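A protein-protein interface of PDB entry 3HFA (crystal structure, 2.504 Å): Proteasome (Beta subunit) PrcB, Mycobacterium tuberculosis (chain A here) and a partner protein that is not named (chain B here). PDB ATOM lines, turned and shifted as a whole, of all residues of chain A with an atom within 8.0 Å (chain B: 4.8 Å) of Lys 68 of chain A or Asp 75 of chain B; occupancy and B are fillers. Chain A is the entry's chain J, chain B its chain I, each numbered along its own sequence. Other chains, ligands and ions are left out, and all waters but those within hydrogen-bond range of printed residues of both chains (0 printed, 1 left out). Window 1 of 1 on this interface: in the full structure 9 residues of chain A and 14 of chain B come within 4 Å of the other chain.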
ATOM      1  N   ARG A  57       1.698  -9.389  23.887  1.00  0.00           N
ATOM      2  CA  ARG A  57       2.534  -8.672  24.837  1.00  0.00           C
ATOM      3  C   ARG A  57       3.903  -9.344  24.988  1.00  0.00           C
ATOM      4  O   ARG A  57       4.951  -8.705  24.867  1.00  0.00           O
ATOM      5  CB  ARG A  57       1.819  -8.605  26.184  1.00  0.00           C
ATOM      6  CG  ARG A  57       2.134  -7.364  26.970  1.00  0.00           C
ATOM      7  CD  ARG A  57       1.169  -7.166  28.124  1.00  0.00           C
ATOM      8  NE  ARG A  57       1.812  -6.309  29.104  1.00  0.00           N
ATOM      9  CZ  ARG A  57       2.399  -6.734  30.218  1.00  0.00           C
ATOM     10  NH1 ARG A  57       2.393  -8.027  30.529  1.00  0.00           N
ATOM     11  NH2 ARG A  57       2.979  -5.852  31.028  1.00  0.00           N
ATOM     12  N   LEU A  58       3.885 -10.645  25.245  1.00  0.00           N
ATOM     13  CA  LEU A  58       5.109 -11.399  25.460  1.00  0.00           C
ATOM     14  C   LEU A  58       5.959 -11.448  24.197  1.00  0.00           C
ATOM     15  O   LEU A  58       7.183 -11.349  24.252  1.00  0.00           O
ATOM     16  CB  LEU A  58       4.777 -12.814  25.905  1.00  0.00           C
ATOM     17  CG  LEU A  58       6.005 -13.622  26.302  1.00  0.00           C
ATOM     18  CD1 LEU A  58       6.860 -12.838  27.302  1.00  0.00           C
ATOM     19  CD2 LEU A  58       5.572 -14.949  26.880  1.00  0.00           C
ATOM     20  N   ALA A  60       6.096  -9.248  21.679  1.00  0.00           N
ATOM     21  CA  ALA A  60       6.728  -7.945  21.461  1.00  0.00           C
ATOM     22  C   ALA A  60       7.918  -7.758  22.402  1.00  0.00           C
ATOM     23  O   ALA A  60       8.963  -7.231  22.010  1.00  0.00           O
ATOM     24  CB  ALA A  60       5.720  -6.830  21.650  1.00  0.00           C
ATOM     25  N   VAL A  61       7.754  -8.199  23.644  1.00  0.00           N
ATOM     26  CA  VAL A  61       8.847  -8.164  24.604  1.00  0.00           C
ATOM     27  C   VAL A  61      10.016  -9.029  24.128  1.00  0.00           C
ATOM     28  O   VAL A  61      11.173  -8.597  24.173  1.00  0.00           O
ATOM     29  CB  VAL A  61       8.380  -8.624  26.003  1.00  0.00           C
ATOM     30  CG1 VAL A  61       9.575  -8.922  26.913  1.00  0.00           C
ATOM     31  CG2 VAL A  61       7.470  -7.569  26.628  1.00  0.00           C
ATOM     32  N   GLU A  62       9.705 -10.240  23.661  1.00  0.00           N
ATOM     33  CA  GLU A  62      10.735 -11.179  23.221  1.00  0.00           C
ATOM     34  C   GLU A  62      11.536 -10.631  22.043  1.00  0.00           C
ATOM     35  O   GLU A  62      12.765 -10.744  22.009  1.00  0.00           O
ATOM     36  CB  GLU A  62      10.124 -12.539  22.870  1.00  0.00           C
ATOM     37  CG  GLU A  62      11.141 -13.545  22.383  1.00  0.00           C
ATOM     38  CD  GLU A  62      10.601 -14.956  22.317  1.00  0.00           C
ATOM     39  OE1 GLU A  62       9.378 -15.148  22.468  1.00  0.00           O
ATOM     40  OE2 GLU A  62      11.411 -15.883  22.121  1.00  0.00           O
ATOM     41  N   LEU A  63      10.837 -10.031  21.085  1.00  0.00           N
ATOM     42  CA  LEU A  63      11.492  -9.455  19.916  1.00  0.00           C
ATOM     43  C   LEU A  63      12.505  -8.369  20.293  1.00  0.00           C
ATOM     44  O   LEU A  63      13.645  -8.373  19.820  1.00  0.00           O
ATOM     45  CB  LEU A  63      10.448  -8.886  18.956  1.00  0.00           C
ATOM     46  CG  LEU A  63      10.120  -9.721  17.715  1.00  0.00           C
ATOM     47  CD1 LEU A  63      10.355 -11.185  17.959  1.00  0.00           C
ATOM     48  CD2 LEU A  63       8.701  -9.482  17.268  1.00  0.00           C
ATOM     49  N   GLU A  64      12.075  -7.442  21.141  1.00  0.00           N
ATOM     50  CA  GLU A  64      12.924  -6.339  21.568  1.00  0.00           C
ATOM     51  C   GLU A  64      14.030  -6.803  22.520  1.00  0.00           C
ATOM     52  O   GLU A  64      15.118  -6.228  22.561  1.00  0.00           O
ATOM     53  CB  GLU A  64      12.069  -5.276  22.241  1.00  0.00           C
ATOM     54  CG  GLU A  64      12.820  -4.015  22.580  1.00  0.00           C
ATOM     55  CD  GLU A  64      11.889  -2.901  23.022  1.00  0.00           C
ATOM     56  OE1 GLU A  64      11.151  -2.362  22.162  1.00  0.00           O
ATOM     57  OE2 GLU A  64      11.894  -2.571  24.228  1.00  0.00           O
ATOM     58  N   HIS A  65      13.735  -7.850  23.280  1.00  0.00           N
ATOM     59  CA  HIS A  65      14.700  -8.464  24.180  1.00  0.00           C
ATOM     60  C   HIS A  65      15.896  -8.984  23.379  1.00  0.00           C
ATOM     61  O   HIS A  65      17.052  -8.721  23.730  1.00  0.00           O
ATOM     62  CB  HIS A  65      14.010  -9.594  24.926  1.00  0.00           C
ATOM     63  CG  HIS A  65      14.877 -10.295  25.917  1.00  0.00           C
ATOM     64  ND1 HIS A  65      15.170  -9.758  27.151  1.00  0.00           N
ATOM     65  CD2 HIS A  65      15.470 -11.514  25.883  1.00  0.00           C
ATOM     66  CE1 HIS A  65      15.929 -10.606  27.825  1.00  0.00           C
ATOM     67  NE2 HIS A  65      16.122 -11.680  27.080  1.00  0.00           N
ATOM     68  N   TYR A  66      15.615  -9.702  22.291  1.00  0.00           N
ATOM     69  CA  TYR A  66      16.672 -10.183  21.413  1.00  0.00           C
ATOM     70  C   TYR A  66      17.497  -9.019  20.853  1.00  0.00           C
ATOM     71  O   TYR A  66      18.735  -9.026  20.886  1.00  0.00           O
ATOM     72  CB  TYR A  66      16.097 -11.012  20.265  1.00  0.00           C
ATOM     73  CG  TYR A  66      17.178 -11.655  19.434  1.00  0.00           C
ATOM     74  CD1 TYR A  66      17.623 -12.943  19.714  1.00  0.00           C
ATOM     75  CD2 TYR A  66      17.777 -10.964  18.384  1.00  0.00           C
ATOM     76  CE1 TYR A  66      18.631 -13.536  18.953  1.00  0.00           C
ATOM     77  CE2 TYR A  66      18.787 -11.541  17.625  1.00  0.00           C
ATOM     78  CZ  TYR A  66      19.212 -12.827  17.911  1.00  0.00           C
ATOM     79  OH  TYR A  66      20.216 -13.398  17.151  1.00  0.00           O
ATOM     80  N   GLU A  67      16.792  -8.015  20.345  1.00  0.00           N
ATOM     81  CA  GLU A  67      17.434  -6.850  19.758  1.00  0.00           C
ATOM     82  C   GLU A  67      18.391  -6.172  20.730  1.00  0.00           C
ATOM     83  O   GLU A  67      19.522  -5.836  20.368  1.00  0.00           O
ATOM     84  CB  GLU A  67      16.387  -5.854  19.273  1.00  0.00           C
ATOM     85  CG  GLU A  67      16.985  -4.647  18.591  1.00  0.00           C
ATOM     86  CD  GLU A  67      15.928  -3.684  18.086  1.00  0.00           C
ATOM     87  OE1 GLU A  67      14.731  -4.027  18.155  1.00  0.00           O
ATOM     88  OE2 GLU A  67      16.294  -2.587  17.616  1.00  0.00           O
ATOM     89  N   LYS A  68      17.944  -6.004  21.967  1.00  0.00           N
ATOM     90  CA  LYS A  68      18.737  -5.364  23.007  1.00  0.00           C
ATOM     91  C   LYS A  68      19.902  -6.212  23.524  1.00  0.00           C
ATOM     92  O   LYS A  68      20.904  -5.669  23.973  1.00  0.00           O
ATOM     93  CB  LYS A  68      17.843  -4.943  24.171  1.00  0.00           C
ATOM     94  CG  LYS A  68      16.871  -3.843  23.829  1.00  0.00           C
ATOM     95  CD  LYS A  68      16.240  -3.266  25.076  1.00  0.00           C
ATOM     96  CE  LYS A  68      15.337  -4.265  25.753  1.00  0.00           C
ATOM     97  NZ  LYS A  68      14.734  -3.714  26.983  1.00  0.00           N
ATOM     98  N   LEU A  69      19.763  -7.534  23.474  1.00  0.00           N
ATOM     99  CA  LEU A  69      20.837  -8.435  23.852  1.00  0.00           C
ATOM    100  C   LEU A  69      21.883  -8.556  22.749  1.00  0.00           C
ATOM    101  O   LEU A  69      23.089  -8.564  23.026  1.00  0.00           O
ATOM    102  CB  LEU A  69      20.284  -9.816  24.200  1.00  0.00           C
ATOM    103  CG  LEU A  69      19.534  -9.975  25.526  1.00  0.00           C
ATOM    104  CD1 LEU A  69      19.012 -11.414  25.673  1.00  0.00           C
ATOM    105  CD2 LEU A  69      20.420  -9.617  26.702  1.00  0.00           C
ATOM    106  N   GLU A  70      21.421  -8.638  21.501  1.00  0.00           N
ATOM    107  CA  GLU A  70      22.305  -9.024  20.398  1.00  0.00           C
ATOM    108  C   GLU A  70      22.700  -7.853  19.508  1.00  0.00           C
ATOM    109  O   GLU A  70      23.558  -7.987  18.631  1.00  0.00           O
ATOM    110  CB  GLU A  70      21.683 -10.149  19.568  1.00  0.00           C
ATOM    111  CG  GLU A  70      21.444 -11.416  20.371  1.00  0.00           C
ATOM    112  CD  GLU A  70      22.687 -11.856  21.119  1.00  0.00           C
ATOM    113  OE1 GLU A  70      23.780 -11.848  20.514  1.00  0.00           O
ATOM    114  OE2 GLU A  70      22.572 -12.214  22.308  1.00  0.00           O
ATOM    115  N   GLY A  71      22.065  -6.710  19.738  1.00  0.00           N
ATOM    116  CA  GLY A  71      22.393  -5.491  19.023  1.00  0.00           C
ATOM    117  C   GLY A  71      21.721  -5.365  17.672  1.00  0.00           C
ATOM    118  O   GLY A  71      21.785  -4.317  17.034  1.00  0.00           O
ATOM    119  N   VAL A  72      21.072  -6.432  17.233  1.00  0.00           N
ATOM    120  CA  VAL A  72      20.421  -6.452  15.929  1.00  0.00           C
ATOM    121  C   VAL A  72      19.082  -7.178  16.062  1.00  0.00           C
ATOM    122  O   VAL A  72      18.922  -8.042  16.927  1.00  0.00           O
ATOM    123  CB  VAL A  72      21.327  -7.164  14.882  1.00  0.00           C
ATOM    124  CG1 VAL A  72      21.597  -8.607  15.299  1.00  0.00           C
ATOM    125  CG2 VAL A  72      20.706  -7.117  13.498  1.00  0.00           C
ATOM    126  N   PRO A  73      18.109  -6.825  15.216  1.00  0.00           N
ATOM    127  CA  PRO A  73      16.818  -7.522  15.280  1.00  0.00           C
ATOM    128  C   PRO A  73      16.917  -8.918  14.680  1.00  0.00           C
ATOM    129  O   PRO A  73      17.798  -9.168  13.855  1.00  0.00           O
ATOM    130  CB  PRO A  73      15.899  -6.662  14.403  1.00  0.00           C
ATOM    131  CG  PRO A  73      16.603  -5.376  14.206  1.00  0.00           C
ATOM    132  CD  PRO A  73      18.080  -5.685  14.289  1.00  0.00           C
ATOM    133  N   SER B  46      24.570   0.944  25.849  1.00  0.00           N
ATOM    134  CA  SER B  46      23.419   0.181  25.412  1.00  0.00           C
ATOM    135  C   SER B  46      22.093   0.632  25.989  1.00  0.00           C
ATOM    136  O   SER B  46      22.030   1.360  26.975  1.00  0.00           O
ATOM    137  CB  SER B  46      23.637  -1.299  25.742  1.00  0.00           C
ATOM    138  OG  SER B  46      22.647  -2.112  25.143  1.00  0.00           O
ATOM    139  N   GLU B  47      21.035   0.165  25.345  1.00  0.00           N
ATOM    140  CA  GLU B  47      19.676   0.450  25.741  1.00  0.00           C
ATOM    141  C   GLU B  47      19.223  -0.627  26.709  1.00  0.00           C
ATOM    142  O   GLU B  47      19.287  -1.808  26.398  1.00  0.00           O
ATOM    143  CB  GLU B  47      18.801   0.412  24.493  1.00  0.00           C
ATOM    144  CG  GLU B  47      17.322   0.283  24.736  1.00  0.00           C
ATOM    145  CD  GLU B  47      16.559   0.124  23.443  1.00  0.00           C
ATOM    146  OE1 GLU B  47      17.204  -0.051  22.393  1.00  0.00           O
ATOM    147  OE2 GLU B  47      15.317   0.167  23.473  1.00  0.00           O
ATOM    148  N   LEU B  48      18.782  -0.220  27.893  1.00  0.00           N
ATOM    149  CA  LEU B  48      18.298  -1.161  28.891  1.00  0.00           C
ATOM    150  C   LEU B  48      16.779  -1.283  28.837  1.00  0.00           C
ATOM    151  O   LEU B  48      16.227  -2.377  28.912  1.00  0.00           O
ATOM    152  CB  LEU B  48      18.702  -0.709  30.289  1.00  0.00           C
ATOM    153  CG  LEU B  48      20.136  -0.911  30.764  1.00  0.00           C
ATOM    154  CD1 LEU B  48      20.248  -0.483  32.211  1.00  0.00           C
ATOM    155  CD2 LEU B  48      20.553  -2.361  30.606  1.00  0.00           C
ATOM    156  N   TYR B  49      16.116  -0.140  28.701  1.00  0.00           N
ATOM    157  CA  TYR B  49      14.662  -0.062  28.661  1.00  0.00           C
ATOM    158  C   TYR B  49      14.199   1.139  27.847  1.00  0.00           C
ATOM    159  O   TYR B  49      15.002   1.783  27.184  1.00  0.00           O
ATOM    160  CB  TYR B  49      14.049  -0.067  30.058  1.00  0.00           C
ATOM    161  CG  TYR B  49      12.755  -0.848  30.116  1.00  0.00           C
ATOM    162  CD1 TYR B  49      12.684  -2.139  29.611  1.00  0.00           C
ATOM    163  CD2 TYR B  49      11.609  -0.303  30.676  1.00  0.00           C
ATOM    164  CE1 TYR B  49      11.513  -2.861  29.654  1.00  0.00           C
ATOM    165  CE2 TYR B  49      10.431  -1.022  30.726  1.00  0.00           C
ATOM    166  CZ  TYR B  49      10.390  -2.300  30.213  1.00  0.00           C
ATOM    167  OH  TYR B  49       9.223  -3.021  30.260  1.00  0.00           O
ATOM    168  N   ARG B  67      25.209  -6.097  31.528  1.00  0.00           N
ATOM    169  CA  ARG B  67      24.294  -5.493  30.567  1.00  0.00           C
ATOM    170  C   ARG B  67      23.121  -6.442  30.259  1.00  0.00           C
ATOM    171  O   ARG B  67      21.956  -6.057  30.329  1.00  0.00           O
ATOM    172  CB  ARG B  67      25.046  -5.129  29.281  1.00  0.00           C
ATOM    173  CG  ARG B  67      24.229  -4.295  28.288  1.00  0.00           C
ATOM    174  CD  ARG B  67      24.946  -4.174  26.949  1.00  0.00           C
ATOM    175  NE  ARG B  67      25.124  -5.480  26.324  1.00  0.00           N
ATOM    176  CZ  ARG B  67      24.267  -6.006  25.457  1.00  0.00           C
ATOM    177  NH1 ARG B  67      23.186  -5.325  25.111  1.00  0.00           N
ATOM    178  NH2 ARG B  67      24.488  -7.203  24.932  1.00  0.00           N
ATOM    179  N   ILE B  71      19.015  -6.100  31.174  1.00  0.00           N
ATOM    180  CA  ILE B  71      17.961  -6.211  30.177  1.00  0.00           C
ATOM    181  C   ILE B  71      16.999  -7.338  30.537  1.00  0.00           C
ATOM    182  O   ILE B  71      15.797  -7.211  30.370  1.00  0.00           O
ATOM    183  CB  ILE B  71      18.528  -6.467  28.782  1.00  0.00           C
ATOM    184  CG1 ILE B  71      19.401  -5.293  28.346  1.00  0.00           C
ATOM    185  CG2 ILE B  71      17.406  -6.689  27.797  1.00  0.00           C
ATOM    186  CD1 ILE B  71      20.085  -5.495  27.024  1.00  0.00           C
ATOM    187  N   GLN B  72      17.538  -8.443  31.035  1.00  0.00           N
ATOM    188  CA  GLN B  72      16.707  -9.533  31.530  1.00  0.00           C
ATOM    189  C   GLN B  72      15.810  -9.039  32.670  1.00  0.00           C
ATOM    190  O   GLN B  72      14.601  -9.270  32.677  1.00  0.00           O
ATOM    191  CB  GLN B  72      17.584 -10.704  31.993  1.00  0.00           C
ATOM    192  CG  GLN B  72      16.823 -11.888  32.571  1.00  0.00           C
ATOM    193  CD  GLN B  72      15.952 -12.586  31.543  1.00  0.00           C
ATOM    194  OE1 GLN B  72      16.209 -12.513  30.342  1.00  0.00           O
ATOM    195  NE2 GLN B  72      14.914 -13.272  32.014  1.00  0.00           N
ATOM    196  N   PHE B  73      16.408  -8.340  33.626  1.00  0.00           N
ATOM    197  CA  PHE B  73      15.673  -7.855  34.785  1.00  0.00           C
ATOM    198  C   PHE B  73      14.576  -6.878  34.363  1.00  0.00           C
ATOM    199  O   PHE B  73      13.417  -7.011  34.773  1.00  0.00           O
ATOM    200  CB  PHE B  73      16.627  -7.171  35.779  1.00  0.00           C
ATOM    201  CG  PHE B  73      15.926  -6.548  36.953  1.00  0.00           C
ATOM    202  CD1 PHE B  73      15.647  -7.298  38.085  1.00  0.00           C
ATOM    203  CD2 PHE B  73      15.512  -5.222  36.913  1.00  0.00           C
ATOM    204  CE1 PHE B  73      14.978  -6.738  39.165  1.00  0.00           C
ATOM    205  CE2 PHE B  73      14.840  -4.667  37.984  1.00  0.00           C
ATOM    206  CZ  PHE B  73      14.575  -5.426  39.112  1.00  0.00           C
ATOM    207  N   ALA B  74      14.952  -5.888  33.558  1.00  0.00           N
ATOM    208  CA  ALA B  74      14.005  -4.880  33.105  1.00  0.00           C
ATOM    209  C   ALA B  74      12.827  -5.497  32.343  1.00  0.00           C
ATOM    210  O   ALA B  74      11.672  -5.231  32.661  1.00  0.00           O
ATOM    211  CB  ALA B  74      14.711  -3.832  32.254  1.00  0.00           C
ATOM    212  N   ASP B  75      13.113  -6.326  31.345  1.00  0.00           N
ATOM    213  CA  ASP B  75      12.043  -6.898  30.529  1.00  0.00           C
ATOM    214  C   ASP B  75      11.106  -7.759  31.366  1.00  0.00           C
ATOM    215  O   ASP B  75       9.888  -7.755  31.154  1.00  0.00           O
ATOM    216  CB  ASP B  75      12.618  -7.695  29.355  1.00  0.00           C
ATOM    217  CG  ASP B  75      13.196  -6.796  28.274  1.00  0.00           C
ATOM    218  OD1 ASP B  75      12.919  -5.580  28.309  1.00  0.00           O
ATOM    219  OD2 ASP B  75      13.919  -7.303  27.392  1.00  0.00           O
ATOM    220  N   THR B  76      11.679  -8.485  32.324  1.00  0.00           N
ATOM    221  CA  THR B  76      10.886  -9.324  33.221  1.00  0.00           C
ATOM    222  C   THR B  76       9.948  -8.493  34.107  1.00  0.00           C
ATOM    223  O   THR B  76       8.753  -8.778  34.199  1.00  0.00           O
ATOM    224  CB  THR B  76      11.790 -10.231  34.077  1.00  0.00           C
ATOM    225  OG1 THR B  76      12.398 -11.216  33.232  1.00  0.00           O
ATOM    226  CG2 THR B  76      10.976 -10.940  35.148  1.00  0.00           C
ATOM    227  N   ARG B  77      10.493  -7.464  34.750  1.00  0.00           N
ATOM    228  CA  ARG B  77       9.686  -6.568  35.570  1.00  0.00           C
ATOM    229  C   ARG B  77       8.568  -5.903  34.776  1.00  0.00           C
ATOM    230  O   ARG B  77       7.416  -5.860  35.217  1.00  0.00           O
ATOM    231  CB  ARG B  77      10.554  -5.484  36.207  1.00  0.00           C
ATOM    232  CG  ARG B  77      11.416  -5.990  37.343  1.00  0.00           C
ATOM    233  CD  ARG B  77      10.577  -6.745  38.357  1.00  0.00           C
ATOM    234  NE  ARG B  77      11.185  -6.673  39.679  1.00  0.00           N
ATOM    235  CZ  ARG B  77      11.052  -5.633  40.491  1.00  0.00           C
ATOM    236  NH1 ARG B  77      10.324  -4.593  40.110  1.00  0.00           N
ATOM    237  NH2 ARG B  77      11.640  -5.633  41.678  1.00  0.00           N
ATOM    238  N   GLY B  78       8.919  -5.368  33.614  1.00  0.00           N
ATOM    239  CA  GLY B  78       7.947  -4.713  32.760  1.00  0.00           C
ATOM    240  C   GLY B  78       6.818  -5.650  32.395  1.00  0.00           C
ATOM    241  O   GLY B  78       5.657  -5.247  32.338  1.00  0.00           O
ATOM    242  N   TYR B  79       7.155  -6.891  32.074  1.00  0.00           N
ATOM    243  CA  TYR B  79       6.137  -7.883  31.771  1.00  0.00           C
ATOM    244  C   TYR B  79       5.305  -8.248  32.996  1.00  0.00           C
ATOM    245  O   TYR B  79       4.090  -8.366  32.920  1.00  0.00           O
ATOM    246  CB  TYR B  79       6.753  -9.133  31.149  1.00  0.00           C
ATOM    247  CG  TYR B  79       5.721 -10.102  30.630  1.00  0.00           C
ATOM    248  CD1 TYR B  79       5.138  -9.918  29.390  1.00  0.00           C
ATOM    249  CD2 TYR B  79       5.320 -11.186  31.387  1.00  0.00           C
ATOM    250  CE1 TYR B  79       4.191 -10.790  28.917  1.00  0.00           C
ATOM    251  CE2 TYR B  79       4.373 -12.063  30.921  1.00  0.00           C
ATOM    252  CZ  TYR B  79       3.812 -11.861  29.684  1.00  0.00           C
ATOM    253  OH  TYR B  79       2.866 -12.731  29.209  1.00  0.00           O
ATOM    254  N   ARG B 212      10.869   4.480  22.861  1.00  0.00           N
ATOM    255  CA  ARG B 212      12.264   4.091  23.028  1.00  0.00           C
ATOM    256  C   ARG B 212      13.075   5.350  22.861  1.00  0.00           C
ATOM    257  O   ARG B 212      13.100   5.951  21.794  1.00  0.00           O
ATOM    258  CB  ARG B 212      12.661   3.042  21.995  1.00  0.00           C
ATOM    259  CG  ARG B 212      11.849   1.768  22.084  1.00  0.00           C
ATOM    260  CD  ARG B 212      12.232   0.784  20.998  1.00  0.00           C
ATOM    261  NE  ARG B 212      13.354  -0.060  21.389  1.00  0.00           N
ATOM    262  CZ  ARG B 212      13.996  -0.875  20.563  1.00  0.00           C
ATOM    263  NH1 ARG B 212      13.632  -0.955  19.294  1.00  0.00           N
ATOM    264  NH2 ARG B 212      15.004  -1.604  21.004  1.00  0.00           N
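Of the 15 printed residues of chain B, 10 touch a printed residue of chain A.
Printed residues of chain B that touch a printed residue of chain A: Glu 47, Leu 48, Tyr 49, Arg 67, Ile 71, Gln 72, Asp 75, Gly 78, Tyr 79 and Arg 212.
Printed residues of chain A that touch a printed residue of chain B: Arg 57, Leu 58, Glu 64, His 65, Glu 67, Lys 68 and Leu 69.
Hydrophobic or aromatic side chains of chain A within 4 Å of the printed part of chain B: Leu 58 and His 65.
Among the printed residues, 15 pairs touch across the chains.
Among the printed residues, Asp or Glu carboxylates within 4 Å of a Lys or Arg side-chain nitrogen of the other chain: Glu 64 of chain A with Arg 212 of chain B, Glu 67 of chain A with Arg 212 of chain B and Lys 68 of chain A with Asp 75 of chain B.
Leu 58 of chain A touches Tyr 79 of chain B.
CG2 of Ile 71 of chain B touches ND1 of His 65 of chain A (3.9 Å).
CD of Lys 68 of chain A touches O of Glu 47 of chain B (3.6 Å).
Tyr 49 of chain B touches Lys 68 of chain A.
Lys 68 of chain A touches Ile 71 of chain B (O to CD1, 3.2 Å).
The backbone carbonyl oxygen (O) of Gly 78 of chain B lies within hydrogen-bond range of the guanidinium group (NH2) of Arg 57 of chain A.
NH1 of Arg 57 of chain A sits at hydrogen-bond distance from O of Tyr 79 of chain B.
The side-chain carboxylate (OE1) of Glu 64 of chain A lies within salt-bridge range of the guanidinium group (NE) of Arg 212 of chain B (3.3 Å).
NE2 of His 65 of chain A sits close to OE1 of Gln 72 of chain B, 3.4 Å away.
A ring nitrogen (ND1) of His 65 of chain A lies within hydrogen-bond range of the side-chain carboxylate (OD2) of Asp 75 of chain B (2.8 Å).
The side-chain carboxylate of Glu 67 of chain A is in salt-bridge range of the guanidinium group of Arg 212 of chain B.
The side-chain amino group (NZ) of Lys 68 of chain A is in hydrogen-bond range of the backbone carbonyl oxygen (O) of Leu 48 of chain B.
The backbone carbonyl oxygen (O) of Lys 68 of chain A lies within hydrogen-bond range of the guanidinium group (NH1) of Arg 67 of chain B (2.6 Å).
NZ of Lys 68 of chain A is in salt-bridge range of OD1 of Asp 75 of chain B, at 2.9 Å.
O of Leu 69 of chain A sits at hydrogen-bond distance from NH2 of Arg 67 of chain B (2.7 Å).
OG of Ser 46 of chain B lies within hydrogen-bond range of NH1 of Arg 67 of chain B, 3.3 Å away.
OE2 of Glu 47 of chain B lies within salt-bridge range of NE of Arg 212 of chain B, 2.9 Å away.
O of Gln 72 of chain B is in hydrogen-bond range of OG1 of Thr 76 of chain B.
Of the printed residues of chain B, Lys 68 of chain A touches Glu 47 (3.6 Å), Leu 48 (2.8 Å), Tyr 49 (3.7 Å), Arg 67 (2.6 Å), Ile 71 (3.2 Å) and Asp 75 (2.9 Å).
No residue of chain A comes within 4 Å of Ala 74 of chain B.
Of the printed residues of chain A, Tyr 79 of chain B touches Arg 57 (3.0 Å) and Leu 58 (3.6 Å).
Printed residues of chain B within 4 Å of Leu 58 of chain A: Tyr 79 (3.6 Å).
Of the printed residues of chain B, Leu 69 of chain A touches Arg 67.
Glu 62 of chain A touches none of the printed residues of chain B.
The nearest residue of chain B that does not touch Lys 68 of chain A is Arg 212 of chain B (4.1 Å).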
